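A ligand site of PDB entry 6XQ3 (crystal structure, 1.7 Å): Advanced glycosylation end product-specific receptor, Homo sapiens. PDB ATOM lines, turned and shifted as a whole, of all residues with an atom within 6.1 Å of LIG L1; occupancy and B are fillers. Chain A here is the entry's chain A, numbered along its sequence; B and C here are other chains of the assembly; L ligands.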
ATOM      1  N   ALA A   2     -11.763  -5.350  23.308  1.00  0.00           N
ATOM      2  CA  ALA A   2     -13.170  -5.722  23.256  1.00  0.00           C
ATOM      3  C   ALA A   2     -13.693  -5.528  21.841  1.00  0.00           C
ATOM      4  O   ALA A   2     -13.000  -5.011  20.979  1.00  0.00           O
ATOM      5  CB  ALA A   2     -14.005  -4.900  24.242  1.00  0.00           C
ATOM      6  N   MET A   3     -14.919  -5.998  21.616  1.00  0.00           N
ATOM      7  CA  MET A   3     -15.629  -5.663  20.388  1.00  0.00           C
ATOM      8  C   MET A   3     -15.844  -4.163  20.279  1.00  0.00           C
ATOM      9  O   MET A   3     -16.276  -3.496  21.234  1.00  0.00           O
ATOM     10  CB  MET A   3     -17.028  -6.344  20.356  1.00  0.00           C
ATOM     11  CG  MET A   3     -16.895  -7.835  20.034  1.00  0.00           C
ATOM     12  SD  MET A   3     -16.680  -7.998  18.237  1.00  0.00           S
ATOM     13  CE  MET A   3     -16.394  -9.724  18.212  1.00  0.00           C
ATOM     14  N   ALA A   4     -15.622  -3.651  19.081  1.00  0.00           N
ATOM     15  CA  ALA A   4     -15.755  -2.240  18.832  1.00  0.00           C
ATOM     16  C   ALA A   4     -16.240  -1.973  17.429  1.00  0.00           C
ATOM     17  O   ALA A   4     -16.079  -2.796  16.535  1.00  0.00           O
ATOM     18  CB  ALA A   4     -14.361  -1.538  19.006  1.00  0.00           C
ATOM     19  N   GLN A   5     -16.755  -0.757  17.212  1.00  0.00           N
ATOM     20  CA  GLN A   5     -17.010  -0.271  15.873  1.00  0.00           C
ATOM     21  C   GLN A   5     -15.708   0.271  15.304  1.00  0.00           C
ATOM     22  O   GLN A   5     -15.109   1.161  15.908  1.00  0.00           O
ATOM     23  CB  GLN A   5     -18.082   0.815  15.907  1.00  0.00           C
ATOM     24  CG  GLN A   5     -18.121   1.675  14.683  1.00  0.00           C
ATOM     25  CD  GLN A   5     -18.763   0.951  13.520  1.00  0.00           C
ATOM     26  OE1 GLN A   5     -19.402  -0.067  13.708  1.00  0.00           O
ATOM     27  NE2 GLN A   5     -18.627   1.507  12.322  1.00  0.00           N
ATOM     28  N   LYS A  20     -23.697   6.694  22.248  1.00  0.00           N
ATOM     29  CA  LYS A  20     -24.960   5.940  22.184  1.00  0.00           C
ATOM     30  C   LYS A  20     -25.710   6.061  23.503  1.00  0.00           C
ATOM     31  O   LYS A  20     -25.129   5.970  24.588  1.00  0.00           O
ATOM     32  CB  LYS A  20     -24.673   4.459  21.863  1.00  0.00           C
ATOM     33  CG  LYS A  20     -24.236   4.244  20.413  1.00  0.00           C
ATOM     34  CD  LYS A  20     -23.780   2.779  20.192  1.00  0.00           C
ATOM     35  CE  LYS A  20     -23.391   2.577  18.706  1.00  0.00           C
ATOM     36  NZ  LYS A  20     -21.934   2.823  18.393  1.00  0.00           N
ATOM     37  N   GLU A  31     -19.635   9.981  30.157  1.00  0.00           N
ATOM     38  CA  GLU A  31     -18.199  10.179  30.240  1.00  0.00           C
ATOM     39  C   GLU A  31     -17.538   9.569  29.015  1.00  0.00           C
ATOM     40  O   GLU A  31     -17.904   8.470  28.613  1.00  0.00           O
ATOM     41  CB  GLU A  31     -17.659   9.448  31.444  1.00  0.00           C
ATOM     42  CG  GLU A  31     -16.442   9.971  31.998  1.00  0.00           C
ATOM     43  CD  GLU A  31     -16.251   9.438  33.417  1.00  0.00           C
ATOM     44  OE1 GLU A  31     -16.286  10.241  34.339  1.00  0.00           O
ATOM     45  OE2 GLU A  31     -16.085   8.204  33.547  1.00  0.00           O
ATOM     46  N   TRP A  32     -16.536  10.246  28.433  1.00  0.00           N
ATOM     47  CA  TRP A  32     -15.710   9.637  27.377  1.00  0.00           C
ATOM     48  C   TRP A  32     -14.336   9.264  27.946  1.00  0.00           C
ATOM     49  O   TRP A  32     -13.846   9.927  28.843  1.00  0.00           O
ATOM     50  CB  TRP A  32     -15.449  10.628  26.230  1.00  0.00           C
ATOM     51  CG  TRP A  32     -16.619  10.779  25.248  1.00  0.00           C
ATOM     52  CD1 TRP A  32     -17.661  11.651  25.365  1.00  0.00           C
ATOM     53  CD2 TRP A  32     -16.867   9.999  24.086  1.00  0.00           C
ATOM     54  NE1 TRP A  32     -18.570  11.457  24.335  1.00  0.00           N
ATOM     55  CE2 TRP A  32     -18.119  10.425  23.547  1.00  0.00           C
ATOM     56  CE3 TRP A  32     -16.227   8.906  23.498  1.00  0.00           C
ATOM     57  CZ2 TRP A  32     -18.642   9.881  22.382  1.00  0.00           C
ATOM     58  CZ3 TRP A  32     -16.712   8.382  22.340  1.00  0.00           C
ATOM     59  CH2 TRP A  32     -17.948   8.856  21.774  1.00  0.00           C
ATOM     60  N   LYS A  33     -13.797   8.146  27.477  1.00  0.00           N
ATOM     61  CA  LYS A  33     -12.437   7.688  27.828  1.00  0.00           C
ATOM     62  C   LYS A  33     -11.718   7.400  26.539  1.00  0.00           C
ATOM     63  O   LYS A  33     -12.256   6.748  25.642  1.00  0.00           O
ATOM     64  CB  LYS A  33     -12.472   6.370  28.722  1.00  0.00           C
ATOM     65  CG  LYS A  33     -12.691   6.694  30.134  1.00  0.00           C
ATOM     66  CD  LYS A  33     -13.100   5.464  30.968  1.00  0.00           C
ATOM     67  CE  LYS A  33     -12.405   4.205  30.564  1.00  0.00           C
ATOM     68  NZ  LYS A  33     -12.529   3.223  31.723  1.00  0.00           N
ATOM     69  N   VAL A  44      -9.847  10.585  30.691  1.00  0.00           N
ATOM     70  CA  VAL A  44     -11.272  10.785  30.777  1.00  0.00           C
ATOM     71  C   VAL A  44     -11.616  12.216  30.343  1.00  0.00           C
ATOM     72  O   VAL A  44     -10.968  13.179  30.768  1.00  0.00           O
ATOM     73  CB  VAL A  44     -11.720  10.547  32.223  1.00  0.00           C
ATOM     74  CG1 VAL A  44     -13.191  10.941  32.329  1.00  0.00           C
ATOM     75  CG2 VAL A  44     -11.502   9.118  32.550  1.00  0.00           C
ATOM     76  N   ARG A  79     -14.110   5.533  23.973  1.00  0.00           N
ATOM     77  CA  ARG A  79     -15.284   4.876  24.566  1.00  0.00           C
ATOM     78  C   ARG A  79     -16.151   5.895  25.257  1.00  0.00           C
ATOM     79  O   ARG A  79     -15.653   6.853  25.836  1.00  0.00           O
ATOM     80  CB  ARG A  79     -14.851   3.861  25.630  1.00  0.00           C
ATOM     81  CG  ARG A  79     -14.152   2.799  25.081  1.00  0.00           C
ATOM     82  CD  ARG A  79     -13.650   1.909  26.266  1.00  0.00           C
ATOM     83  NE  ARG A  79     -13.228   0.675  25.714  1.00  0.00           N
ATOM     84  CZ  ARG A  79     -12.835  -0.373  26.447  1.00  0.00           C
ATOM     85  NH1 ARG A  79     -12.796  -0.320  27.774  1.00  0.00           N
ATOM     86  NH2 ARG A  79     -12.468  -1.470  25.819  1.00  0.00           N
ATOM     87  N   CYS A  80     -17.473   5.648  25.219  1.00  0.00           N
ATOM     88  CA  CYS A  80     -18.432   6.453  25.969  1.00  0.00           C
ATOM     89  C   CYS A  80     -19.270   5.569  26.867  1.00  0.00           C
ATOM     90  O   CYS A  80     -19.549   4.428  26.525  1.00  0.00           O
ATOM     91  CB  CYS A  80     -19.417   7.227  24.984  1.00  0.00           C
ATOM     92  SG  CYS A  80     -20.078   8.678  25.910  1.00  0.00           S
ATOM     93  N   GLN A  81     -19.616   6.094  28.040  1.00  0.00           N
ATOM     94  CA  GLN A  81     -20.590   5.433  28.893  1.00  0.00           C
ATOM     95  C   GLN A  81     -21.599   6.469  29.285  1.00  0.00           C
ATOM     96  O   GLN A  81     -21.205   7.522  29.821  1.00  0.00           O
ATOM     97  CB  GLN A  81     -19.919   4.831  30.130  1.00  0.00           C
ATOM     98  CG  GLN A  81     -20.946   4.278  31.135  1.00  0.00           C
ATOM     99  CD  GLN A  81     -20.339   3.344  32.125  1.00  0.00           C
ATOM    100  OE1 GLN A  81     -19.399   3.703  32.845  1.00  0.00           O
ATOM    101  NE2 GLN A  81     -20.877   2.119  32.191  1.00  0.00           N
ATOM    102  N   LYS A  91     -23.071   1.650  26.536  1.00  0.00           N
ATOM    103  CA  LYS A  91     -21.650   1.783  26.174  1.00  0.00           C
ATOM    104  C   LYS A  91     -21.456   2.010  24.679  1.00  0.00           C
ATOM    105  O   LYS A  91     -22.163   1.442  23.843  1.00  0.00           O
ATOM    106  CB  LYS A  91     -20.898   0.533  26.577  1.00  0.00           C
ATOM    107  CG  LYS A  91     -20.731   0.356  28.104  1.00  0.00           C
ATOM    108  CD  LYS A  91     -20.166  -1.073  28.306  1.00  0.00           C
ATOM    109  CE  LYS A  91     -19.621  -1.298  29.657  1.00  0.00           C
ATOM    110  NZ  LYS A  91     -20.474  -0.751  30.740  1.00  0.00           N
ATOM    111  N   SER A  92     -20.402   2.792  24.322  1.00  0.00           N
ATOM    112  CA  SER A  92     -20.017   2.990  22.941  1.00  0.00           C
ATOM    113  C   SER A  92     -18.517   2.699  22.891  1.00  0.00           C
ATOM    114  O   SER A  92     -17.809   3.170  23.760  1.00  0.00           O
ATOM    115  CB  SER A  92     -20.250   4.418  22.441  1.00  0.00           C
ATOM    116  OG  SER A  92     -21.670   4.773  22.604  1.00  0.00           O
ATOM    117  N   ASN A  93     -18.079   1.903  21.916  1.00  0.00           N
ATOM    118  CA  ASN A  93     -16.654   1.509  21.850  1.00  0.00           C
ATOM    119  C   ASN A  93     -16.231   1.638  20.409  1.00  0.00           C
ATOM    120  O   ASN A  93     -16.735   0.916  19.541  1.00  0.00           O
ATOM    121  CB  ASN A  93     -16.482   0.071  22.403  1.00  0.00           C
ATOM    122  CG  ASN A  93     -15.015  -0.299  22.633  1.00  0.00           C
ATOM    123  OD1 ASN A  93     -14.192   0.572  22.912  1.00  0.00           O
ATOM    124  ND2 ASN A  93     -14.695  -1.563  22.497  1.00  0.00           N
ATOM    125  N   TYR A  94     -15.219   2.484  20.141  1.00  0.00           N
ATOM    126  CA  TYR A  94     -14.774   2.775  18.788  1.00  0.00           C
ATOM    127  C   TYR A  94     -13.268   2.495  18.693  1.00  0.00           C
ATOM    128  O   TYR A  94     -12.529   2.915  19.587  1.00  0.00           O
ATOM    129  CB  TYR A  94     -14.966   4.229  18.412  1.00  0.00           C
ATOM    130  CG  TYR A  94     -16.435   4.649  18.447  1.00  0.00           C
ATOM    131  CD1 TYR A  94     -17.253   4.361  17.384  1.00  0.00           C
ATOM    132  CD2 TYR A  94     -16.952   5.251  19.563  1.00  0.00           C
ATOM    133  CE1 TYR A  94     -18.600   4.734  17.422  1.00  0.00           C
ATOM    134  CE2 TYR A  94     -18.340   5.677  19.595  1.00  0.00           C
ATOM    135  CZ  TYR A  94     -19.092   5.386  18.505  1.00  0.00           C
ATOM    136  OH  TYR A  94     -20.440   5.698  18.553  1.00  0.00           O
ATOM    137  N   LYS B 155     -19.084  -5.267  14.067  1.00  0.00           N
ATOM    138  CA  LYS B 155     -18.193  -4.993  15.189  1.00  0.00           C
ATOM    139  C   LYS B 155     -16.992  -5.940  15.150  1.00  0.00           C
ATOM    140  O   LYS B 155     -17.082  -7.096  14.711  1.00  0.00           O
ATOM    141  CB  LYS B 155     -18.938  -5.166  16.548  1.00  0.00           C
ATOM    142  CG  LYS B 155     -20.146  -4.220  16.726  1.00  0.00           C
ATOM    143  CD  LYS B 155     -19.922  -2.727  16.695  1.00  0.00           C
ATOM    144  CE  LYS B 155     -21.208  -1.909  16.343  1.00  0.00           C
ATOM    145  NZ  LYS B 155     -21.416  -1.797  14.839  1.00  0.00           N
ATOM    146  N   LYS C  33      -8.324  -7.351  34.735  1.00  0.00           N
ATOM    147  CA  LYS C  33      -8.090  -6.798  33.393  1.00  0.00           C
ATOM    148  C   LYS C  33      -6.650  -6.386  33.312  1.00  0.00           C
ATOM    149  O   LYS C  33      -6.129  -5.735  34.220  1.00  0.00           O
ATOM    150  CB  LYS C  33      -9.018  -5.536  33.105  1.00  0.00           C
ATOM    151  CG  LYS C  33     -10.360  -5.954  32.664  1.00  0.00           C
ATOM    152  CD  LYS C  33     -11.388  -4.808  32.734  1.00  0.00           C
ATOM    153  CE  LYS C  33     -10.832  -3.475  32.351  1.00  0.00           C
ATOM    154  NZ  LYS C  33     -12.010  -2.570  32.011  1.00  0.00           N
ATOM    155  N   GLN C  81     -11.495  -5.823  39.840  1.00  0.00           N
ATOM    156  CA  GLN C  81     -12.735  -5.291  40.381  1.00  0.00           C
ATOM    157  C   GLN C  81     -13.439  -6.430  41.055  1.00  0.00           C
ATOM    158  O   GLN C  81     -13.664  -7.472  40.413  1.00  0.00           O
ATOM    159  CB  GLN C  81     -13.610  -4.701  39.272  1.00  0.00           C
ATOM    160  CG  GLN C  81     -15.000  -4.289  39.788  1.00  0.00           C
ATOM    161  CD  GLN C  81     -15.709  -3.361  38.861  1.00  0.00           C
ATOM    162  OE1 GLN C  81     -15.922  -3.677  37.684  1.00  0.00           O
ATOM    163  NE2 GLN C  81     -16.106  -2.194  39.373  1.00  0.00           N
HETATM  164  C1  LIG L   1     -16.334   6.172  30.726  1.00  0.00           C
HETATM  165  C2  LIG L   1     -16.453   5.254  31.749  1.00  0.00           C
HETATM  166  C3  LIG L   1     -16.577   3.915  31.408  1.00  0.00           C
HETATM  167  C4  LIG L   1     -16.573   3.514  30.080  1.00  0.00           C
HETATM  168  C5  LIG L   1     -16.463   4.463  29.064  1.00  0.00           C
HETATM  169  C6  LIG L   1     -16.335   5.800  29.391  1.00  0.00           C
HETATM  170  C7  LIG L   1     -16.799   1.744  31.360  1.00  0.00           C
HETATM  171  C8  LIG L   1     -16.729   2.172  30.027  1.00  0.00           C
HETATM  172  C9  LIG L   1     -16.786   1.354  28.714  1.00  0.00           C
HETATM  173  C10 LIG L   1     -16.222   0.092  28.685  1.00  0.00           C
HETATM  174  C11 LIG L   1     -16.233  -0.698  27.541  1.00  0.00           C
HETATM  175  C12 LIG L   1     -16.803  -0.220  26.360  1.00  0.00           C
HETATM  176  C13 LIG L   1     -17.395   1.070  26.347  1.00  0.00           C
HETATM  177  C14 LIG L   1     -17.413   1.861  27.520  1.00  0.00           C
HETATM  178  C15 LIG L   1     -16.951   0.336  31.966  1.00  0.00           C
HETATM  179  C16 LIG L   1     -16.931  -3.396  26.087  1.00  0.00           C
HETATM  180  C17 LIG L   1     -17.815  -3.774  27.090  1.00  0.00           C
HETATM  181  C18 LIG L   1     -19.029  -4.380  26.759  1.00  0.00           C
HETATM  182  C19 LIG L   1     -19.360  -4.600  25.424  1.00  0.00           C
HETATM  183  C20 LIG L   1     -18.475  -4.222  24.421  1.00  0.00           C
HETATM  184  C21 LIG L   1     -17.259  -3.625  24.754  1.00  0.00           C
HETATM  185  C22 LIG L   1     -19.203  -3.329  22.369  1.00  0.00           C
HETATM  186  C23 LIG L   1     -19.754  -2.249  23.042  1.00  0.00           C
HETATM  187  C24 LIG L   1     -20.164  -1.185  22.301  1.00  0.00           C
HETATM  188  C25 LIG L   1     -19.976  -1.181  20.889  1.00  0.00           C
HETATM  189  C26 LIG L   1     -19.407  -2.254  20.227  1.00  0.00           C
HETATM  190  C27 LIG L   1     -19.043  -3.333  20.988  1.00  0.00           C
HETATM  191  C28 LIG L   1     -15.578  -2.736  26.436  1.00  0.00           C
HETATM  192  C29 LIG L   1     -20.427   0.015  20.077  1.00  0.00           C
HETATM  193  N1  LIG L   1     -16.705   2.831  32.176  1.00  0.00           N
HETATM  194  O1  LIG L   1     -16.529   0.119  33.144  1.00  0.00           O
HETATM  195  O2  LIG L   1     -17.501  -0.590  31.345  1.00  0.00           O
HETATM  196  O3  LIG L   1     -15.643  -1.982  27.626  1.00  0.00           O
HETATM  197  O4  LIG L   1     -18.776  -4.460  23.074  1.00  0.00           O
HETATM  198  O5  LIG L   1     -20.251   1.085  20.568  1.00  0.00           O
HETATM  199  O6  LIG L   1     -20.992   0.001  18.933  1.00  0.00           O
HETATM  200  C1  LG2 L   2     -12.500  -5.769  35.710  1.00  0.00           C
HETATM  201  C2  LG2 L   2     -13.547  -4.920  35.421  1.00  0.00           C
HETATM  202  C3  LG2 L   2     -13.406  -3.579  35.752  1.00  0.00           C
HETATM  203  C4  LG2 L   2     -12.243  -3.111  36.346  1.00  0.00           C
HETATM  204  C5  LG2 L   2     -11.203  -3.992  36.638  1.00  0.00           C
HETATM  205  C6  LG2 L   2     -11.331  -5.329  36.311  1.00  0.00           C
HETATM  206  C7  LG2 L   2     -13.640  -1.436  36.086  1.00  0.00           C
HETATM  207  C8  LG2 L   2     -12.375  -1.786  36.579  1.00  0.00           C
HETATM  208  C9  LG2 L   2     -11.282  -0.905  37.252  1.00  0.00           C
HETATM  209  C10 LG2 L   2     -11.124   0.397  36.815  1.00  0.00           C
HETATM  210  C11 LG2 L   2     -10.161   1.246  37.371  1.00  0.00           C
HETATM  211  C12 LG2 L   2      -9.308   0.781  38.364  1.00  0.00           C
HETATM  212  C13 LG2 L   2      -9.444  -0.551  38.834  1.00  0.00           C
HETATM  213  C14 LG2 L   2     -10.435  -1.398  38.307  1.00  0.00           C
HETATM  214  C15 LG2 L   2     -14.367  -0.079  36.034  1.00  0.00           C
HETATM  215  C16 LG2 L   2      -9.383   3.946  38.764  1.00  0.00           C
HETATM  216  C17 LG2 L   2     -10.697   4.195  39.144  1.00  0.00           C
HETATM  217  C18 LG2 L   2     -10.966   4.717  40.419  1.00  0.00           C
HETATM  218  C19 LG2 L   2      -9.925   4.978  41.308  1.00  0.00           C
HETATM  219  C20 LG2 L   2      -8.617   4.726  40.919  1.00  0.00           C
HETATM  220  C21 LG2 L   2      -8.345   4.216  39.651  1.00  0.00           C
HETATM  221  C22 LG2 L   2      -7.009   3.884  42.419  1.00  0.00           C
HETATM  222  C23 LG2 L   2      -7.756   2.731  42.573  1.00  0.00           C
HETATM  223  C24 LG2 L   2      -7.177   1.678  43.207  1.00  0.00           C
HETATM  224  C25 LG2 L   2      -5.826   1.763  43.651  1.00  0.00           C
HETATM  225  C26 LG2 L   2      -5.076   2.913  43.484  1.00  0.00           C
HETATM  226  C27 LG2 L   2      -5.694   3.977  42.882  1.00  0.00           C
HETATM  227  C28 LG2 L   2      -9.062   3.383  37.362  1.00  0.00           C
HETATM  228  C29 LG2 L   2      -5.194   0.575  44.338  1.00  0.00           C
HETATM  229  N1  LG2 L   2     -14.237  -2.550  35.598  1.00  0.00           N
HETATM  230  O1  LG2 L   2     -15.258   0.113  35.162  1.00  0.00           O
HETATM  231  O2  LG2 L   2     -14.122   0.829  36.847  1.00  0.00           O
HETATM  232  O3  LG2 L   2     -10.092   2.568  36.871  1.00  0.00           O
HETATM  233  O4  LG2 L   2      -7.550   5.011  41.796  1.00  0.00           O
HETATM  234  O5  LG2 L   2      -5.471  -0.501  43.911  1.00  0.00           O
HETATM  235  O6  LG2 L   2      -4.409   0.602  45.344  1.00  0.00           O
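NZ of Lys 91 sits close to NE2 of Gln 81 of chain A.
The side-chain sulfur of Cys 80 sits close to the indole nitrogen of Trp 32 (3.5 Å).
The backbone NH (N) of Lys 20 sits at hydrogen-bond distance from the side-chain hydroxyl (OG) of Ser 92 (2.8 Å).
The backbone carbonyl oxygen (O) of Gln 81 of chain A sits at hydrogen-bond distance from the backbone NH (N) of Glu 31 (2.9 Å).
The side-chain amino group (NZ) of Lys 20 is in hydrogen-bond range of the side-chain hydroxyl (OH) of Tyr 94.
The backbone NH (N) of Ser 92 lies within hydrogen-bond range of the backbone carbonyl oxygen (O) of Cys 80.
The backbone carbonyl oxygen (O) of Asn 93 lies within hydrogen-bond range of the backbone NH (N) of Gln 5, 2.9 Å away.
The side-chain amino group of Lys 155 of chain B lies within hydrogen-bond range of the side-chain amide oxygen of Gln 5.
O4 of LIG L1 sits close to O of Met 3.
CB of Ala 2 touches C28 of LIG L1, at 3.5 Å.
Ala 4 touches LIG L1 (CA to C26, 3.9 Å).
Glu 31 touches LIG L1.
Lys 33 of chain A touches LIG L1 (CD to C1, 3.3 Å).
Cys 80 touches LIG L1.
CA of Ser 92 touches O5 of LIG L1, at 3.1 Å.
Lys 155 of chain B touches LIG L1 (CE to O6, 3.2 Å).
Hydrophobic or aromatic side chains that line LIG L1: Ala 2 and Met 3.
13 residues have an atom within 4 Å of LIG L1: Ala 2, Met 3, Ala 4, Lys 20, Glu 31, Lys 33 of chain A, Arg 79, Cys 80, Gln 81 of chain A, Lys 91, Ser 92, Asn 93 and Lys 155 of chain B.
Along chain A the residues within 4 Å of LIG L1 span positions 2 to 93.
The nearest printed residue that does not touch LIG L1 is Trp 32 (4.3 Å).
The side-chain amino group (NZ) of Lys 20 lies within salt-bridge range of an oxygen (O6) of LIG L1.
An oxygen (O2) of LIG L1 is in salt-bridge range of the side-chain amino group (NZ) of Lys 91 (3.0 Å).
NH1 of Arg 79 is in hydrogen-bond range of O3 of LIG L1 (3.3 Å).
The backbone NH (N) of Asn 93 sits at hydrogen-bond distance from an oxygen (O5) of LIG L1, 2.7 Å away.
A nitrogen (N1) of LIG L1 lies within hydrogen-bond range of the side-chain amide oxygen (OE1) of Gln 81 of chain A (2.9 Å).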
